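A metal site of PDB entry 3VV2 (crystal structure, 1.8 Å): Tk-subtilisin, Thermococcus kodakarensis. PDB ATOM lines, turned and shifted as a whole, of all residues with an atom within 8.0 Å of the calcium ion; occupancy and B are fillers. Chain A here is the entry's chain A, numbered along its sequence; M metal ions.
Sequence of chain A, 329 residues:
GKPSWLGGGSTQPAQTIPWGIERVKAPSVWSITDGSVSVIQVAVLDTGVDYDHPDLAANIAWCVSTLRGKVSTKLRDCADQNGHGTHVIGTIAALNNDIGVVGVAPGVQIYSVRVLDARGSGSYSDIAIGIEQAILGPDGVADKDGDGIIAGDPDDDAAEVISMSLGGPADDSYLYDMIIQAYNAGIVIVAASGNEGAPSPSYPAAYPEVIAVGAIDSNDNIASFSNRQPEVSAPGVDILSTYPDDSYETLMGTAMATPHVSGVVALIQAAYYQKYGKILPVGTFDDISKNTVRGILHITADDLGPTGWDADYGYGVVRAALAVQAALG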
ATOM      1  N   GLN A  12     -21.228 -37.459  27.079  1.00  0.00           N
ATOM      2  CA  GLN A  12     -20.547 -36.297  27.687  1.00  0.00           C
ATOM      3  C   GLN A  12     -20.351 -36.400  29.185  1.00  0.00           C
ATOM      4  O   GLN A  12     -21.341 -36.499  29.937  1.00  0.00           O
ATOM      5  CB  GLN A  12     -21.287 -34.999  27.391  1.00  0.00           C
ATOM      6  CG  GLN A  12     -21.244 -34.590  25.962  1.00  0.00           C
ATOM      7  CD  GLN A  12     -19.848 -34.218  25.494  1.00  0.00           C
ATOM      8  OE1 GLN A  12     -19.087 -33.533  26.209  1.00  0.00           O
ATOM      9  NE2 GLN A  12     -19.509 -34.648  24.277  1.00  0.00           N
ATOM     10  N   PRO A  13     -19.098 -36.353  29.641  1.00  0.00           N
ATOM     11  CA  PRO A  13     -18.728 -36.453  31.057  1.00  0.00           C
ATOM     12  C   PRO A  13     -19.087 -35.171  31.816  1.00  0.00           C
ATOM     13  O   PRO A  13     -19.285 -34.132  31.174  1.00  0.00           O
ATOM     14  CB  PRO A  13     -17.208 -36.659  30.998  1.00  0.00           C
ATOM     15  CG  PRO A  13     -16.763 -35.954  29.755  1.00  0.00           C
ATOM     16  CD  PRO A  13     -17.935 -36.073  28.771  1.00  0.00           C
ATOM     17  N   ALA A  14     -19.171 -35.229  33.151  1.00  0.00           N
ATOM     18  CA  ALA A  14     -19.599 -34.064  33.928  1.00  0.00           C
ATOM     19  C   ALA A  14     -18.485 -33.024  33.944  1.00  0.00           C
ATOM     20  O   ALA A  14     -17.303 -33.390  33.869  1.00  0.00           O
ATOM     21  CB  ALA A  14     -19.947 -34.480  35.360  1.00  0.00           C
ATOM     22  N   GLN A  15     -18.850 -31.749  34.096  1.00  0.00           N
ATOM     23  CA  GLN A  15     -17.857 -30.683  33.880  1.00  0.00           C
ATOM     24  C   GLN A  15     -16.750 -30.804  34.885  1.00  0.00           C
ATOM     25  O   GLN A  15     -16.991 -31.080  36.040  1.00  0.00           O
ATOM     26  CB  GLN A  15     -18.456 -29.277  33.972  1.00  0.00           C
ATOM     27  CG  GLN A  15     -17.425 -28.158  33.658  1.00  0.00           C
ATOM     28  CD  GLN A  15     -18.067 -26.830  33.484  1.00  0.00           C
ATOM     29  OE1 GLN A  15     -18.634 -26.538  32.427  1.00  0.00           O
ATOM     30  NE2 GLN A  15     -18.044 -26.027  34.546  1.00  0.00           N
ATOM     31  N   THR A  16     -15.531 -30.559  34.447  1.00  0.00           N
ATOM     32  CA  THR A  16     -14.425 -30.387  35.418  1.00  0.00           C
ATOM     33  C   THR A  16     -13.681 -29.079  35.127  1.00  0.00           C
ATOM     34  O   THR A  16     -13.803 -28.555  34.035  1.00  0.00           O
ATOM     35  CB  THR A  16     -13.474 -31.528  35.321  1.00  0.00           C
ATOM     36  OG1 THR A  16     -12.658 -31.571  36.489  1.00  0.00           O
ATOM     37  CG2 THR A  16     -12.610 -31.415  34.090  1.00  0.00           C
ATOM     38  N   HIS A  53     -19.134 -28.752  18.513  1.00  0.00           N
ATOM     39  CA  HIS A  53     -18.893 -29.290  19.819  1.00  0.00           C
ATOM     40  C   HIS A  53     -19.857 -28.748  20.822  1.00  0.00           C
ATOM     41  O   HIS A  53     -20.114 -27.548  20.871  1.00  0.00           O
ATOM     42  CB  HIS A  53     -17.468 -28.953  20.286  1.00  0.00           C
ATOM     43  CG  HIS A  53     -17.023 -29.750  21.475  1.00  0.00           C
ATOM     44  ND1 HIS A  53     -15.946 -30.608  21.424  1.00  0.00           N
ATOM     45  CD2 HIS A  53     -17.444 -29.753  22.756  1.00  0.00           C
ATOM     46  CE1 HIS A  53     -15.750 -31.150  22.618  1.00  0.00           C
ATOM     47  NE2 HIS A  53     -16.649 -30.632  23.447  1.00  0.00           N
ATOM     48  N   PRO A  54     -20.401 -29.647  21.675  1.00  0.00           N
ATOM     49  CA  PRO A  54     -21.397 -29.141  22.624  1.00  0.00           C
ATOM     50  C   PRO A  54     -20.837 -28.123  23.664  1.00  0.00           C
ATOM     51  O   PRO A  54     -21.601 -27.343  24.195  1.00  0.00           O
ATOM     52  CB  PRO A  54     -21.851 -30.404  23.346  1.00  0.00           C
ATOM     53  CG  PRO A  54     -21.768 -31.464  22.305  1.00  0.00           C
ATOM     54  CD  PRO A  54     -20.427 -31.107  21.598  1.00  0.00           C
ATOM     55  N   ASP A  55     -19.547 -28.208  23.973  1.00  0.00           N
ATOM     56  CA  ASP A  55     -18.954 -27.351  24.998  1.00  0.00           C
ATOM     57  C   ASP A  55     -18.327 -26.121  24.370  1.00  0.00           C
ATOM     58  O   ASP A  55     -17.823 -25.265  25.120  1.00  0.00           O
ATOM     59  CB  ASP A  55     -17.936 -28.098  25.870  1.00  0.00           C
ATOM     60  CG  ASP A  55     -17.981 -27.693  27.350  1.00  0.00           C
ATOM     61  OD1 ASP A  55     -18.948 -27.006  27.747  1.00  0.00           O
ATOM     62  OD2 ASP A  55     -17.000 -27.999  28.130  1.00  0.00           O
ATOM     63  N   LEU A  56     -18.451 -25.991  23.041  1.00  0.00           N
ATOM     64  CA  LEU A  56     -17.966 -24.810  22.272  1.00  0.00           C
ATOM     65  C   LEU A  56     -18.999 -24.037  21.430  1.00  0.00           C
ATOM     66  O   LEU A  56     -18.838 -22.853  21.195  1.00  0.00           O
ATOM     67  CB  LEU A  56     -16.834 -25.199  21.322  1.00  0.00           C
ATOM     68  CG  LEU A  56     -15.577 -25.898  21.811  1.00  0.00           C
ATOM     69  CD1 LEU A  56     -14.534 -26.128  20.618  1.00  0.00           C
ATOM     70  CD2 LEU A  56     -14.916 -25.106  23.041  1.00  0.00           C
ATOM     71  N   ALA A  93     -12.451 -20.610  25.862  1.00  0.00           N
ATOM     72  CA  ALA A  93     -13.890 -20.352  25.776  1.00  0.00           C
ATOM     73  C   ALA A  93     -14.848 -21.538  26.037  1.00  0.00           C
ATOM     74  O   ALA A  93     -16.056 -21.386  25.937  1.00  0.00           O
ATOM     75  CB  ALA A  93     -14.171 -19.575  24.435  1.00  0.00           C
ATOM     76  N   ALA A  94     -14.337 -22.691  26.445  1.00  0.00           N
ATOM     77  CA  ALA A  94     -15.280 -23.790  26.717  1.00  0.00           C
ATOM     78  C   ALA A  94     -16.380 -23.282  27.713  1.00  0.00           C
ATOM     79  O   ALA A  94     -16.087 -22.566  28.689  1.00  0.00           O
ATOM     80  CB  ALA A  94     -14.525 -25.020  27.205  1.00  0.00           C
ATOM     81  N   LEU A  95     -17.630 -23.616  27.414  1.00  0.00           N
ATOM     82  CA  LEU A  95     -18.837 -23.128  28.117  1.00  0.00           C
ATOM     83  C   LEU A  95     -18.887 -23.572  29.556  1.00  0.00           C
ATOM     84  O   LEU A  95     -18.422 -24.684  29.882  1.00  0.00           O
ATOM     85  CB  LEU A  95     -20.118 -23.621  27.343  1.00  0.00           C
ATOM     86  CG  LEU A  95     -20.230 -23.018  25.940  1.00  0.00           C
ATOM     87  CD1 LEU A  95     -20.991 -23.847  24.850  1.00  0.00           C
ATOM     88  CD2 LEU A  95     -20.777 -21.589  26.017  1.00  0.00           C
ATOM     89  N   ASN A  96     -19.380 -22.714  30.443  1.00  0.00           N
ATOM     90  CA  ASN A  96     -19.465 -23.038  31.835  1.00  0.00           C
ATOM     91  C   ASN A  96     -20.856 -23.686  32.011  1.00  0.00           C
ATOM     92  O   ASN A  96     -21.852 -23.006  32.010  1.00  0.00           O
ATOM     93  CB  ASN A  96     -19.264 -21.826  32.777  1.00  0.00           C
ATOM     94  CG  ASN A  96     -19.215 -22.237  34.262  1.00  0.00           C
ATOM     95  OD1 ASN A  96     -19.410 -23.382  34.560  1.00  0.00           O
ATOM     96  ND2 ASN A  96     -18.919 -21.313  35.167  1.00  0.00           N
ATOM     97  N   ASN A  97     -20.860 -24.991  32.157  1.00  0.00           N
ATOM     98  CA  ASN A  97     -22.077 -25.734  32.216  1.00  0.00           C
ATOM     99  C   ASN A  97     -21.900 -27.089  32.888  1.00  0.00           C
ATOM    100  O   ASN A  97     -20.974 -27.293  33.607  1.00  0.00           O
ATOM    101  CB  ASN A  97     -22.644 -25.879  30.818  1.00  0.00           C
ATOM    102  CG  ASN A  97     -21.695 -26.543  29.868  1.00  0.00           C
ATOM    103  OD1 ASN A  97     -20.790 -27.224  30.273  1.00  0.00           O
ATOM    104  ND2 ASN A  97     -21.931 -26.368  28.601  1.00  0.00           N
ATOM    105  N   ASP A  98     -22.858 -27.976  32.681  1.00  0.00           N
ATOM    106  CA  ASP A  98     -22.715 -29.373  33.138  1.00  0.00           C
ATOM    107  C   ASP A  98     -21.818 -30.406  32.505  1.00  0.00           C
ATOM    108  O   ASP A  98     -21.699 -31.539  33.013  1.00  0.00           O
ATOM    109  CB  ASP A  98     -24.149 -29.918  33.073  1.00  0.00           C
ATOM    110  CG  ASP A  98     -25.065 -29.250  34.065  1.00  0.00           C
ATOM    111  OD1 ASP A  98     -24.605 -28.944  35.198  1.00  0.00           O
ATOM    112  OD2 ASP A  98     -26.252 -29.073  33.719  1.00  0.00           O
ATOM    113  N   ILE A  99     -21.218 -30.029  31.378  1.00  0.00           N
ATOM    114  CA  ILE A  99     -20.385 -30.936  30.630  1.00  0.00           C
ATOM    115  C   ILE A  99     -18.947 -30.457  30.415  1.00  0.00           C
ATOM    116  O   ILE A  99     -18.668 -29.244  30.462  1.00  0.00           O
ATOM    117  CB  ILE A  99     -21.057 -31.330  29.244  1.00  0.00           C
ATOM    118  CG1 ILE A  99     -21.404 -30.079  28.400  1.00  0.00           C
ATOM    119  CG2 ILE A  99     -22.356 -32.128  29.499  1.00  0.00           C
ATOM    120  CD1 ILE A  99     -21.445 -30.349  26.851  1.00  0.00           C
ATOM    121  N   GLY A 100     -18.048 -31.427  30.266  1.00  0.00           N
ATOM    122  CA  GLY A 100     -16.726 -31.203  29.675  1.00  0.00           C
ATOM    123  C   GLY A 100     -15.734 -30.445  30.513  1.00  0.00           C
ATOM    124  O   GLY A 100     -15.339 -30.900  31.582  1.00  0.00           O
ATOM    125  N   VAL A 101     -15.244 -29.334  29.962  1.00  0.00           N
ATOM    126  CA  VAL A 101     -14.318 -28.459  30.674  1.00  0.00           C
ATOM    127  C   VAL A 101     -14.867 -27.048  30.684  1.00  0.00           C
ATOM    128  O   VAL A 101     -16.003 -26.801  30.278  1.00  0.00           O
ATOM    129  CB  VAL A 101     -12.943 -28.485  30.033  1.00  0.00           C
ATOM    130  CG1 VAL A 101     -12.252 -29.831  30.343  1.00  0.00           C
ATOM    131  CG2 VAL A 101     -13.005 -28.240  28.496  1.00  0.00           C
ATOM    132  N   VAL A 102     -14.098 -26.077  31.175  1.00  0.00           N
ATOM    133  CA  VAL A 102     -14.545 -24.675  31.052  1.00  0.00           C
ATOM    134  C   VAL A 102     -13.341 -23.767  30.694  1.00  0.00           C
ATOM    135  O   VAL A 102     -12.231 -24.083  31.087  1.00  0.00           O
ATOM    136  CB  VAL A 102     -15.201 -24.254  32.452  1.00  0.00           C
ATOM    137  CG1 VAL A 102     -14.214 -24.465  33.643  1.00  0.00           C
ATOM    138  CG2 VAL A 102     -15.702 -22.817  32.454  1.00  0.00           C
ATOM    139  N   GLY A 103     -13.592 -22.719  29.905  1.00  0.00           N
ATOM    140  CA  GLY A 103     -12.535 -21.824  29.463  1.00  0.00           C
ATOM    141  C   GLY A 103     -12.256 -20.719  30.445  1.00  0.00           C
ATOM    142  O   GLY A 103     -12.974 -20.506  31.409  1.00  0.00           O
ATOM    143  N   PRO A 106     -15.405 -18.080  29.678  1.00  0.00           N
ATOM    144  CA  PRO A 106     -16.270 -19.108  29.139  1.00  0.00           C
ATOM    145  C   PRO A 106     -17.557 -18.603  28.488  1.00  0.00           C
ATOM    146  O   PRO A 106     -18.314 -19.428  27.981  1.00  0.00           O
ATOM    147  CB  PRO A 106     -16.600 -19.983  30.360  1.00  0.00           C
ATOM    148  CG  PRO A 106     -16.477 -19.161  31.524  1.00  0.00           C
ATOM    149  CD  PRO A 106     -15.289 -18.181  31.152  1.00  0.00           C
ATOM    150  N   THR A 242     -11.214 -29.259  25.068  1.00  0.00           N
ATOM    151  CA  THR A 242     -12.067 -29.857  24.002  1.00  0.00           C
ATOM    152  C   THR A 242     -11.231 -30.457  22.834  1.00  0.00           C
ATOM    153  O   THR A 242     -10.081 -30.037  22.593  1.00  0.00           O
ATOM    154  CB  THR A 242     -13.041 -28.766  23.476  1.00  0.00           C
ATOM    155  OG1 THR A 242     -12.294 -27.583  23.224  1.00  0.00           O
ATOM    156  CG2 THR A 242     -14.078 -28.453  24.502  1.00  0.00           C
ATOM    157  N   TYR A 248     -12.711 -34.779  24.254  1.00  0.00           N
ATOM    158  CA  TYR A 248     -11.697 -34.045  25.003  1.00  0.00           C
ATOM    159  C   TYR A 248     -10.360 -34.753  24.926  1.00  0.00           C
ATOM    160  O   TYR A 248     -10.254 -35.958  24.577  1.00  0.00           O
ATOM    161  CB  TYR A 248     -12.210 -33.983  26.499  1.00  0.00           C
ATOM    162  CG  TYR A 248     -13.578 -33.407  26.587  1.00  0.00           C
ATOM    163  CD1 TYR A 248     -14.694 -34.222  26.453  1.00  0.00           C
ATOM    164  CD2 TYR A 248     -13.754 -32.023  26.673  1.00  0.00           C
ATOM    165  CE1 TYR A 248     -15.963 -33.692  26.446  1.00  0.00           C
ATOM    166  CE2 TYR A 248     -15.029 -31.478  26.656  1.00  0.00           C
ATOM    167  CZ  TYR A 248     -16.134 -32.313  26.561  1.00  0.00           C
ATOM    168  OH  TYR A 248     -17.375 -31.760  26.574  1.00  0.00           O
HETATM  169 CA    CA M   1     -18.326 -27.035  30.043  1.00  0.00          CA
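NE2 of Gln 15 is in hydrogen-bond range of OD1 of Asn 96.
The backbone NH (N) of Gln 15 lies within hydrogen-bond range of the backbone carbonyl oxygen (O) of Asp 98.
Six residues have an atom within 4 Å of the calcium ion: Gln 15, Asp 55, Leu 95, Asn 97, Ile 99 and Val 101.
The nearest printed residue that does not touch the calcium ion is Gly 100 (4.3 Å).
The backbone carbonyl oxygen (O) of Ile 99 binds the calcium ion (2.3 Å).
O of Val 101 is bound to the calcium ion (2.3 Å).
The calcium ion is bound by the backbone carbonyl oxygen (O) of Leu 95, at 2.4 Å.
The calcium ion is bound by the side-chain carboxylate (OD1) of Asp 55, at 2.4 Å.
OE1 of Gln 15 binds the calcium ion (2.5 Å).
The calcium ion is bound by the side-chain amide oxygen (OD1) of Asn 97, 2.5 Å away.
The side-chain carboxylate (OD2) of Asp 55 is bound to the calcium ion (2.5 Å).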
